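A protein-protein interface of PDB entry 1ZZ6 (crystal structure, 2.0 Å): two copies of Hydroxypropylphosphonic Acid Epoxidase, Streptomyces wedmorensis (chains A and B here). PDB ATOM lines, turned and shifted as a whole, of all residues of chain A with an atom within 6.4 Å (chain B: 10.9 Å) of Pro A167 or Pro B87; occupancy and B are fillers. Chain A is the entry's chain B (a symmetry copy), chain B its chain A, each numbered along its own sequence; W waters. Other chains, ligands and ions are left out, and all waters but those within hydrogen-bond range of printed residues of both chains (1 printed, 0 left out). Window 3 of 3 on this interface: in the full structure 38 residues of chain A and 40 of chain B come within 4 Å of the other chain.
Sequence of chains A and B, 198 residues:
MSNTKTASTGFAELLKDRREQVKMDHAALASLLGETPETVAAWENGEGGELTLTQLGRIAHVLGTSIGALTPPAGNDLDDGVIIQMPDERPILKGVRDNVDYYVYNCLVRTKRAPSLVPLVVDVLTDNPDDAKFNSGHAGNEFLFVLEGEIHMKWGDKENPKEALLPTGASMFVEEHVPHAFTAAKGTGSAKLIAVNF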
ATOM      1  N   VAL A 146      13.890 -16.666  30.767  1.00  0.00           N
ATOM      2  CA  VAL A 146      12.632 -16.070  31.217  1.00  0.00           C
ATOM      3  C   VAL A 146      11.511 -17.069  30.953  1.00  0.00           C
ATOM      4  O   VAL A 146      11.137 -17.289  29.803  1.00  0.00           O
ATOM      5  CB  VAL A 146      12.298 -14.774  30.451  1.00  0.00           C
ATOM      6  CG1 VAL A 146      10.968 -14.196  30.967  1.00  0.00           C
ATOM      7  CG2 VAL A 146      13.415 -13.772  30.610  1.00  0.00           C
ATOM      8  N   GLY A 149       6.206 -14.037  31.773  1.00  0.00           N
ATOM      9  CA  GLY A 149       6.251 -12.594  31.926  1.00  0.00           C
ATOM     10  C   GLY A 149       7.436 -11.874  31.310  1.00  0.00           C
ATOM     11  O   GLY A 149       8.152 -12.420  30.472  1.00  0.00           O
ATOM     12  N   GLU A 150       7.627 -10.627  31.723  1.00  0.00           N
ATOM     13  CA  GLU A 150       8.724  -9.803  31.236  1.00  0.00           C
ATOM     14  C   GLU A 150       9.619  -9.483  32.414  1.00  0.00           C
ATOM     15  O   GLU A 150       9.138  -9.087  33.473  1.00  0.00           O
ATOM     16  CB  GLU A 150       8.203  -8.494  30.644  1.00  0.00           C
ATOM     17  CG  GLU A 150       7.294  -8.646  29.438  1.00  0.00           C
ATOM     18  CD  GLU A 150       6.641  -7.327  29.037  1.00  0.00           C
ATOM     19  OE1 GLU A 150       7.377  -6.351  28.769  1.00  0.00           O
ATOM     20  OE2 GLU A 150       5.390  -7.268  28.995  1.00  0.00           O
ATOM     21  N   ILE A 151      10.922  -9.644  32.224  1.00  0.00           N
ATOM     22  CA  ILE A 151      11.890  -9.373  33.274  1.00  0.00           C
ATOM     23  C   ILE A 151      12.674  -8.102  32.985  1.00  0.00           C
ATOM     24  O   ILE A 151      13.053  -7.843  31.844  1.00  0.00           O
ATOM     25  CB  ILE A 151      12.906 -10.533  33.410  1.00  0.00           C
ATOM     26  CG1 ILE A 151      12.214 -11.784  33.968  1.00  0.00           C
ATOM     27  CG2 ILE A 151      14.073 -10.105  34.295  1.00  0.00           C
ATOM     28  CD1 ILE A 151      11.845 -11.686  35.439  1.00  0.00           C
ATOM     29  N   LEU A 165      15.321  -5.035  29.135  1.00  0.00           N
ATOM     30  CA  LEU A 165      14.013  -5.637  29.301  1.00  0.00           C
ATOM     31  C   LEU A 165      14.017  -6.897  28.463  1.00  0.00           C
ATOM     32  O   LEU A 165      14.269  -6.844  27.261  1.00  0.00           O
ATOM     33  CB  LEU A 165      12.914  -4.679  28.837  1.00  0.00           C
ATOM     34  CG  LEU A 165      12.500  -3.665  29.912  1.00  0.00           C
ATOM     35  CD1 LEU A 165      13.706  -2.841  30.350  1.00  0.00           C
ATOM     36  CD2 LEU A 165      11.393  -2.766  29.368  1.00  0.00           C
ATOM     37  N   LEU A 166      13.751  -8.029  29.105  1.00  0.00           N
ATOM     38  CA  LEU A 166      13.767  -9.319  28.428  1.00  0.00           C
ATOM     39  C   LEU A 166      12.406 -10.006  28.373  1.00  0.00           C
ATOM     40  O   LEU A 166      11.767 -10.220  29.399  1.00  0.00           O
ATOM     41  CB  LEU A 166      14.769 -10.238  29.127  1.00  0.00           C
ATOM     42  CG  LEU A 166      16.091  -9.553  29.472  1.00  0.00           C
ATOM     43  CD1 LEU A 166      16.974 -10.498  30.256  1.00  0.00           C
ATOM     44  CD2 LEU A 166      16.780  -9.098  28.196  1.00  0.00           C
ATOM     45  N   PRO A 167      11.950 -10.364  27.164  1.00  0.00           N
ATOM     46  CA  PRO A 167      10.661 -11.033  26.983  1.00  0.00           C
ATOM     47  C   PRO A 167      10.746 -12.513  27.323  1.00  0.00           C
ATOM     48  O   PRO A 167      11.833 -13.061  27.508  1.00  0.00           O
ATOM     49  CB  PRO A 167      10.370 -10.813  25.508  1.00  0.00           C
ATOM     50  CG  PRO A 167      11.745 -10.904  24.905  1.00  0.00           C
ATOM     51  CD  PRO A 167      12.555 -10.041  25.858  1.00  0.00           C
ATOM     52  N   THR A 168       9.588 -13.153  27.402  1.00  0.00           N
ATOM     53  CA  THR A 168       9.522 -14.571  27.701  1.00  0.00           C
ATOM     54  C   THR A 168      10.305 -15.308  26.623  1.00  0.00           C
ATOM     55  O   THR A 168      10.155 -15.022  25.435  1.00  0.00           O
ATOM     56  CB  THR A 168       8.066 -15.069  27.684  1.00  0.00           C
ATOM     57  OG1 THR A 168       7.287 -14.291  28.597  1.00  0.00           O
ATOM     58  CG2 THR A 168       7.993 -16.530  28.092  1.00  0.00           C
ATOM     59  N   GLY A 169      11.148 -16.245  27.039  1.00  0.00           N
ATOM     60  CA  GLY A 169      11.924 -16.996  26.076  1.00  0.00           C
ATOM     61  C   GLY A 169      13.336 -16.495  25.851  1.00  0.00           C
ATOM     62  O   GLY A 169      14.122 -17.168  25.183  1.00  0.00           O
ATOM     63  N   ALA A 170      13.671 -15.320  26.377  1.00  0.00           N
ATOM     64  CA  ALA A 170      15.024 -14.809  26.203  1.00  0.00           C
ATOM     65  C   ALA A 170      15.945 -15.545  27.180  1.00  0.00           C
ATOM     66  O   ALA A 170      15.500 -15.993  28.237  1.00  0.00           O
ATOM     67  CB  ALA A 170      15.070 -13.323  26.492  1.00  0.00           C
ATOM     68  N   SER A 171      17.220 -15.670  26.836  1.00  0.00           N
ATOM     69  CA  SER A 171      18.150 -16.324  27.750  1.00  0.00           C
ATOM     70  C   SER A 171      19.335 -15.408  27.984  1.00  0.00           C
ATOM     71  O   SER A 171      19.632 -14.546  27.168  1.00  0.00           O
ATOM     72  CB  SER A 171      18.603 -17.690  27.204  1.00  0.00           C
ATOM     73  OG  SER A 171      19.331 -17.592  25.992  1.00  0.00           O
ATOM     74  N   ILE B  84      23.194 -11.374  26.373  1.00  0.00           N
ATOM     75  CA  ILE B  84      21.776 -11.677  26.279  1.00  0.00           C
ATOM     76  C   ILE B  84      21.369 -12.117  24.889  1.00  0.00           C
ATOM     77  O   ILE B  84      21.903 -11.630  23.896  1.00  0.00           O
ATOM     78  CB  ILE B  84      20.931 -10.437  26.641  1.00  0.00           C
ATOM     79  CG1 ILE B  84      21.195 -10.040  28.091  1.00  0.00           C
ATOM     80  CG2 ILE B  84      19.451 -10.719  26.400  1.00  0.00           C
ATOM     81  CD1 ILE B  84      20.489  -8.779  28.519  1.00  0.00           C
ATOM     82  N   GLN B  85      20.420 -13.042  24.827  1.00  0.00           N
ATOM     83  CA  GLN B  85      19.914 -13.537  23.554  1.00  0.00           C
ATOM     84  C   GLN B  85      18.396 -13.448  23.533  1.00  0.00           C
ATOM     85  O   GLN B  85      17.722 -14.017  24.399  1.00  0.00           O
ATOM     86  CB  GLN B  85      20.313 -14.994  23.326  1.00  0.00           C
ATOM     87  CG  GLN B  85      19.663 -15.595  22.085  1.00  0.00           C
ATOM     88  CD  GLN B  85      19.548 -17.105  22.150  1.00  0.00           C
ATOM     89  OE1 GLN B  85      18.765 -17.650  22.935  1.00  0.00           O
ATOM     90  NE2 GLN B  85      20.328 -17.790  21.325  1.00  0.00           N
ATOM     91  N   MET B  86      17.862 -12.737  22.543  1.00  0.00           N
ATOM     92  CA  MET B  86      16.417 -12.602  22.395  1.00  0.00           C
ATOM     93  C   MET B  86      15.936 -13.848  21.654  1.00  0.00           C
ATOM     94  O   MET B  86      16.673 -14.423  20.841  1.00  0.00           O
ATOM     95  CB  MET B  86      16.084 -11.336  21.609  1.00  0.00           C
ATOM     96  CG  MET B  86      16.549 -10.060  22.303  1.00  0.00           C
ATOM     97  SD  MET B  86      15.797  -9.836  23.924  1.00  0.00           S
ATOM     98  CE  MET B  86      15.371  -8.093  23.843  1.00  0.00           C
ATOM     99  N   PRO B  87      14.693 -14.277  21.907  1.00  0.00           N
ATOM    100  CA  PRO B  87      14.151 -15.478  21.253  1.00  0.00           C
ATOM    101  C   PRO B  87      14.235 -15.592  19.736  1.00  0.00           C
ATOM    102  O   PRO B  87      14.172 -16.698  19.200  1.00  0.00           O
ATOM    103  CB  PRO B  87      12.710 -15.544  21.768  1.00  0.00           C
ATOM    104  CG  PRO B  87      12.398 -14.114  22.127  1.00  0.00           C
ATOM    105  CD  PRO B  87      13.675 -13.629  22.749  1.00  0.00           C
ATOM    106  N   ASP B  88      14.395 -14.469  19.043  1.00  0.00           N
ATOM    107  CA  ASP B  88      14.469 -14.486  17.584  1.00  0.00           C
ATOM    108  C   ASP B  88      15.848 -14.881  17.052  1.00  0.00           C
ATOM    109  O   ASP B  88      15.975 -15.369  15.927  1.00  0.00           O
ATOM    110  CB  ASP B  88      14.090 -13.104  17.032  1.00  0.00           C
ATOM    111  CG  ASP B  88      15.193 -12.072  17.223  1.00  0.00           C
ATOM    112  OD1 ASP B  88      16.139 -12.040  16.405  1.00  0.00           O
ATOM    113  OD2 ASP B  88      15.121 -11.298  18.197  1.00  0.00           O
ATOM    114  N   GLU B  89      16.872 -14.678  17.871  1.00  0.00           N
ATOM    115  CA  GLU B  89      18.248 -14.967  17.483  1.00  0.00           C
ATOM    116  C   GLU B  89      18.677 -16.424  17.609  1.00  0.00           C
ATOM    117  O   GLU B  89      19.740 -16.798  17.122  1.00  0.00           O
ATOM    118  CB  GLU B  89      19.203 -14.105  18.310  1.00  0.00           C
ATOM    119  CG  GLU B  89      18.788 -12.652  18.452  1.00  0.00           C
ATOM    120  CD  GLU B  89      19.740 -11.876  19.350  1.00  0.00           C
ATOM    121  OE1 GLU B  89      20.870 -11.581  18.908  1.00  0.00           O
ATOM    122  OE2 GLU B  89      19.366 -11.575  20.503  1.00  0.00           O
ATOM    123  N   ARG B  90      17.865 -17.247  18.261  1.00  0.00           N
ATOM    124  CA  ARG B  90      18.215 -18.655  18.450  1.00  0.00           C
ATOM    125  C   ARG B  90      18.529 -19.421  17.177  1.00  0.00           C
ATOM    126  O   ARG B  90      17.734 -19.425  16.242  1.00  0.00           O
ATOM    127  CB  ARG B  90      17.079 -19.433  19.122  1.00  0.00           C
ATOM    128  CG  ARG B  90      16.581 -18.920  20.445  1.00  0.00           C
ATOM    129  CD  ARG B  90      15.421 -19.798  20.907  1.00  0.00           C
ATOM    130  NE  ARG B  90      14.817 -19.294  22.129  1.00  0.00           N
ATOM    131  CZ  ARG B  90      13.704 -19.784  22.656  1.00  0.00           C
ATOM    132  NH1 ARG B  90      13.088 -20.795  22.052  1.00  0.00           N
ATOM    133  NH2 ARG B  90      13.213 -19.266  23.777  1.00  0.00           N
ATOM    134  N   PRO B  91      19.698 -20.071  17.111  1.00  0.00           N
ATOM    135  CA  PRO B  91      19.898 -20.808  15.862  1.00  0.00           C
ATOM    136  C   PRO B  91      19.034 -22.060  16.024  1.00  0.00           C
ATOM    137  O   PRO B  91      18.939 -22.608  17.128  1.00  0.00           O
ATOM    138  CB  PRO B  91      21.401 -21.110  15.868  1.00  0.00           C
ATOM    139  CG  PRO B  91      21.762 -21.092  17.308  1.00  0.00           C
ATOM    140  CD  PRO B  91      20.967 -19.923  17.841  1.00  0.00           C
ATOM    141  N   ILE B  92      18.371 -22.490  14.955  1.00  0.00           N
ATOM    142  CA  ILE B  92      17.523 -23.674  15.041  1.00  0.00           C
ATOM    143  C   ILE B  92      18.154 -24.807  14.262  1.00  0.00           C
ATOM    144  O   ILE B  92      18.481 -24.652  13.090  1.00  0.00           O
ATOM    145  CB  ILE B  92      16.102 -23.423  14.477  1.00  0.00           C
ATOM    146  CG1 ILE B  92      15.350 -22.417  15.350  1.00  0.00           C
ATOM    147  CG2 ILE B  92      15.331 -24.719  14.436  1.00  0.00           C
ATOM    148  CD1 ILE B  92      15.745 -20.984  15.117  1.00  0.00           C
ATOM    149  N   TYR B 105      16.284 -28.601  17.955  1.00  0.00           N
ATOM    150  CA  TYR B 105      17.160 -27.947  18.916  1.00  0.00           C
ATOM    151  C   TYR B 105      17.189 -26.430  18.754  1.00  0.00           C
ATOM    152  O   TYR B 105      17.763 -25.917  17.797  1.00  0.00           O
ATOM    153  CB  TYR B 105      18.587 -28.491  18.781  1.00  0.00           C
ATOM    154  CG  TYR B 105      18.710 -29.966  19.087  1.00  0.00           C
ATOM    155  CD1 TYR B 105      18.910 -30.896  18.066  1.00  0.00           C
ATOM    156  CD2 TYR B 105      18.608 -30.435  20.395  1.00  0.00           C
ATOM    157  CE1 TYR B 105      19.004 -32.257  18.341  1.00  0.00           C
ATOM    158  CE2 TYR B 105      18.697 -31.789  20.681  1.00  0.00           C
ATOM    159  CZ  TYR B 105      18.895 -32.696  19.654  1.00  0.00           C
ATOM    160  OH  TYR B 105      18.971 -34.039  19.944  1.00  0.00           O
ATOM    161  N   ASN B 106      16.561 -25.716  19.685  1.00  0.00           N
ATOM    162  CA  ASN B 106      16.549 -24.254  19.641  1.00  0.00           C
ATOM    163  C   ASN B 106      17.638 -23.806  20.593  1.00  0.00           C
ATOM    164  O   ASN B 106      17.438 -23.780  21.808  1.00  0.00           O
ATOM    165  CB  ASN B 106      15.194 -23.719  20.104  1.00  0.00           C
ATOM    166  CG  ASN B 106      14.043 -24.329  19.335  1.00  0.00           C
ATOM    167  OD1 ASN B 106      13.624 -25.459  19.600  1.00  0.00           O
ATOM    168  ND2 ASN B 106      13.540 -23.596  18.359  1.00  0.00           N
ATOM    169  N   CYS B 107      18.789 -23.448  20.038  1.00  0.00           N
ATOM    170  CA  CYS B 107      19.927 -23.058  20.856  1.00  0.00           C
ATOM    171  C   CYS B 107      19.781 -21.729  21.572  1.00  0.00           C
ATOM    172  O   CYS B 107      19.466 -20.707  20.957  1.00  0.00           O
ATOM    173  CB  CYS B 107      21.181 -23.052  19.997  1.00  0.00           C
ATOM    174  SG  CYS B 107      21.451 -24.643  19.197  1.00  0.00           S
ATOM    175  N   LEU B 108      20.019 -21.757  22.880  1.00  0.00           N
ATOM    176  CA  LEU B 108      19.927 -20.567  23.724  1.00  0.00           C
ATOM    177  C   LEU B 108      21.305 -19.885  23.801  1.00  0.00           C
ATOM    178  O   LEU B 108      22.240 -20.304  23.132  1.00  0.00           O
ATOM    179  CB  LEU B 108      19.416 -20.969  25.114  1.00  0.00           C
ATOM    180  CG  LEU B 108      18.007 -21.578  25.058  1.00  0.00           C
ATOM    181  CD1 LEU B 108      17.545 -22.007  26.427  1.00  0.00           C
ATOM    182  CD2 LEU B 108      17.030 -20.540  24.466  1.00  0.00           C
ATOM    183  N   VAL B 109      21.429 -18.840  24.606  1.00  0.00           N
ATOM    184  CA  VAL B 109      22.687 -18.091  24.704  1.00  0.00           C
ATOM    185  C   VAL B 109      23.958 -18.906  24.994  1.00  0.00           C
ATOM    186  O   VAL B 109      23.940 -19.839  25.792  1.00  0.00           O
ATOM    187  CB  VAL B 109      22.581 -16.990  25.782  1.00  0.00           C
ATOM    188  CG1 VAL B 109      22.623 -17.609  27.165  1.00  0.00           C
ATOM    189  CG2 VAL B 109      23.729 -15.982  25.620  1.00  0.00           C
ATOM    190  N   VAL B 121      16.461 -25.436  24.120  1.00  0.00           N
ATOM    191  CA  VAL B 121      15.071 -25.739  24.385  1.00  0.00           C
ATOM    192  C   VAL B 121      14.924 -26.863  23.385  1.00  0.00           C
ATOM    193  O   VAL B 121      15.109 -26.653  22.193  1.00  0.00           O
ATOM    194  CB  VAL B 121      14.134 -24.600  23.997  1.00  0.00           C
ATOM    195  CG1 VAL B 121      12.694 -25.074  24.100  1.00  0.00           C
ATOM    196  CG2 VAL B 121      14.355 -23.419  24.923  1.00  0.00           C
ATOM    197  N   ASP B 123      12.676 -29.520  21.408  1.00  0.00           N
ATOM    198  CA  ASP B 123      11.310 -29.878  21.049  1.00  0.00           C
ATOM    199  C   ASP B 123      11.332 -31.389  20.851  1.00  0.00           C
ATOM    200  O   ASP B 123      12.065 -31.880  20.000  1.00  0.00           O
ATOM    201  CB  ASP B 123      10.888 -29.207  19.741  1.00  0.00           C
ATOM    202  CG  ASP B 123      10.804 -27.694  19.848  1.00  0.00           C
ATOM    203  OD1 ASP B 123      10.353 -27.180  20.897  1.00  0.00           O
ATOM    204  OD2 ASP B 123      11.174 -27.019  18.863  1.00  0.00           O
ATOM    205  N   LYS B 192       8.358 -30.478  25.571  1.00  0.00           N
ATOM    206  CA  LYS B 192       9.515 -29.605  25.449  1.00  0.00           C
ATOM    207  C   LYS B 192      10.411 -29.700  26.676  1.00  0.00           C
ATOM    208  O   LYS B 192       9.938 -29.846  27.796  1.00  0.00           O
ATOM    209  CB  LYS B 192       9.069 -28.153  25.243  1.00  0.00           C
ATOM    210  CG  LYS B 192       8.280 -27.922  23.973  1.00  0.00           C
ATOM    211  CD  LYS B 192       8.107 -26.430  23.671  1.00  0.00           C
ATOM    212  CE  LYS B 192       7.440 -26.218  22.306  1.00  0.00           C
ATOM    213  NZ  LYS B 192       7.556 -24.822  21.808  1.00  0.00           N
HETATM  214  O   HOH W   1      16.311 -17.257  23.615  1.00  0.00           O
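Of chain B, only Met B86 and Pro B87 come within 4 Å of Pro A167. Pro B87 touches just these residues of chain A: Pro A167 (3.97 Å) and Ala A170 (3.9 Å). No residue of chain B comes within 4 Å of Val A146. No residue of chain B comes within 4 Å of Gly A149. Leu A166 touches just one residue of chain B: Ile B84 (3.6 Å). Thr A168 touches none of the printed residues of chain B. Gly A169 touches just one residue of chain B: Arg B90 (2.7 Å). Ala A170 touches just these residues of chain B: Gln B85 (3.3 Å) and Pro B87 (3.9 Å). Printed residues of chain B within 4 Å of Leu A165: Met B86 (3.8 Å). Printed residues of chain A within 4 Å of Leu B108: Ser A171. Printed residues of chain A within 4 Å of Val B109: Ser A171. Glu B89 touches none of the printed residues of chain A. The nearest residue of chain B that does not touch Pro A167 is Gln B85 (6.7 Å).
The side-chain amide nitrogen (NE2) of Gln B85 is in hydrogen-bond range of the backbone carbonyl oxygen (O) of Cys B107 (3.1 Å). OE1 of Gln B85 lies within hydrogen-bond range of N of Val B109 (3.4 Å). The backbone NH of Met B86 lies within hydrogen-bond range of the side-chain carboxylate of Glu B89 (2.8 Å). O of Val A146 lies within hydrogen-bond range of N of Gly A169 (3.0 Å). The backbone NH (N) of Val A146 lies within hydrogen-bond range of the backbone carbonyl oxygen (O) of Ala A170 (3.1 Å). O of Ile A151 is in hydrogen-bond range of N of Leu A166.
Among the printed residues, pairs that only touch across the chains: Leu A165 with Met B86 (3.8 Å), Leu A166 with Ile B84 (3.6 Å), Pro A167 with Met B86 (3.8 Å), Pro A167 with Pro B87 (3.97 Å), Ala A170 with Gln B85 (3.3 Å), Ala A170 with Pro B87 (3.9 Å), Ser A171 with Ile B84 (3.7 Å) and Ser A171 with Leu B108 (3.5 Å).
No position is printed for both chains.
The backbone NH (N) of Gln B85 sits at hydrogen-bond distance from the backbone carbonyl oxygen (O) of Ser A171, at 2.9 Å. The guanidinium group (NH2) of Arg B90 sits at hydrogen-bond distance from the backbone carbonyl oxygen (O) of Gly A169 (2.7 Å). OG of Ser A171 sits at hydrogen-bond distance from N of Val B109.
Water W1 lies within hydrogen-bond range of OE1 of Gln B85, O of Gly A169 and NE of Arg B90.
Hydrophobic or aromatic side chains of chain A that line the printed part of chain B: Leu A166, Pro A167 and Ala A170. Along chain A the printed residues that touch a printed residue of chain B span positions 165 to 171. Of the 17 printed residues of chain B, 7 touch a printed residue of chain A. Hydrophobic or aromatic side chains of chain B that line the printed part of chain A: Ile B84, Met B86, Pro B87, Leu B108 and Val B109. Along chain B the printed residues that touch a printed residue of chain A span positions 84 to 109. Among the printed residues, 11 pairs touch across the chains.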
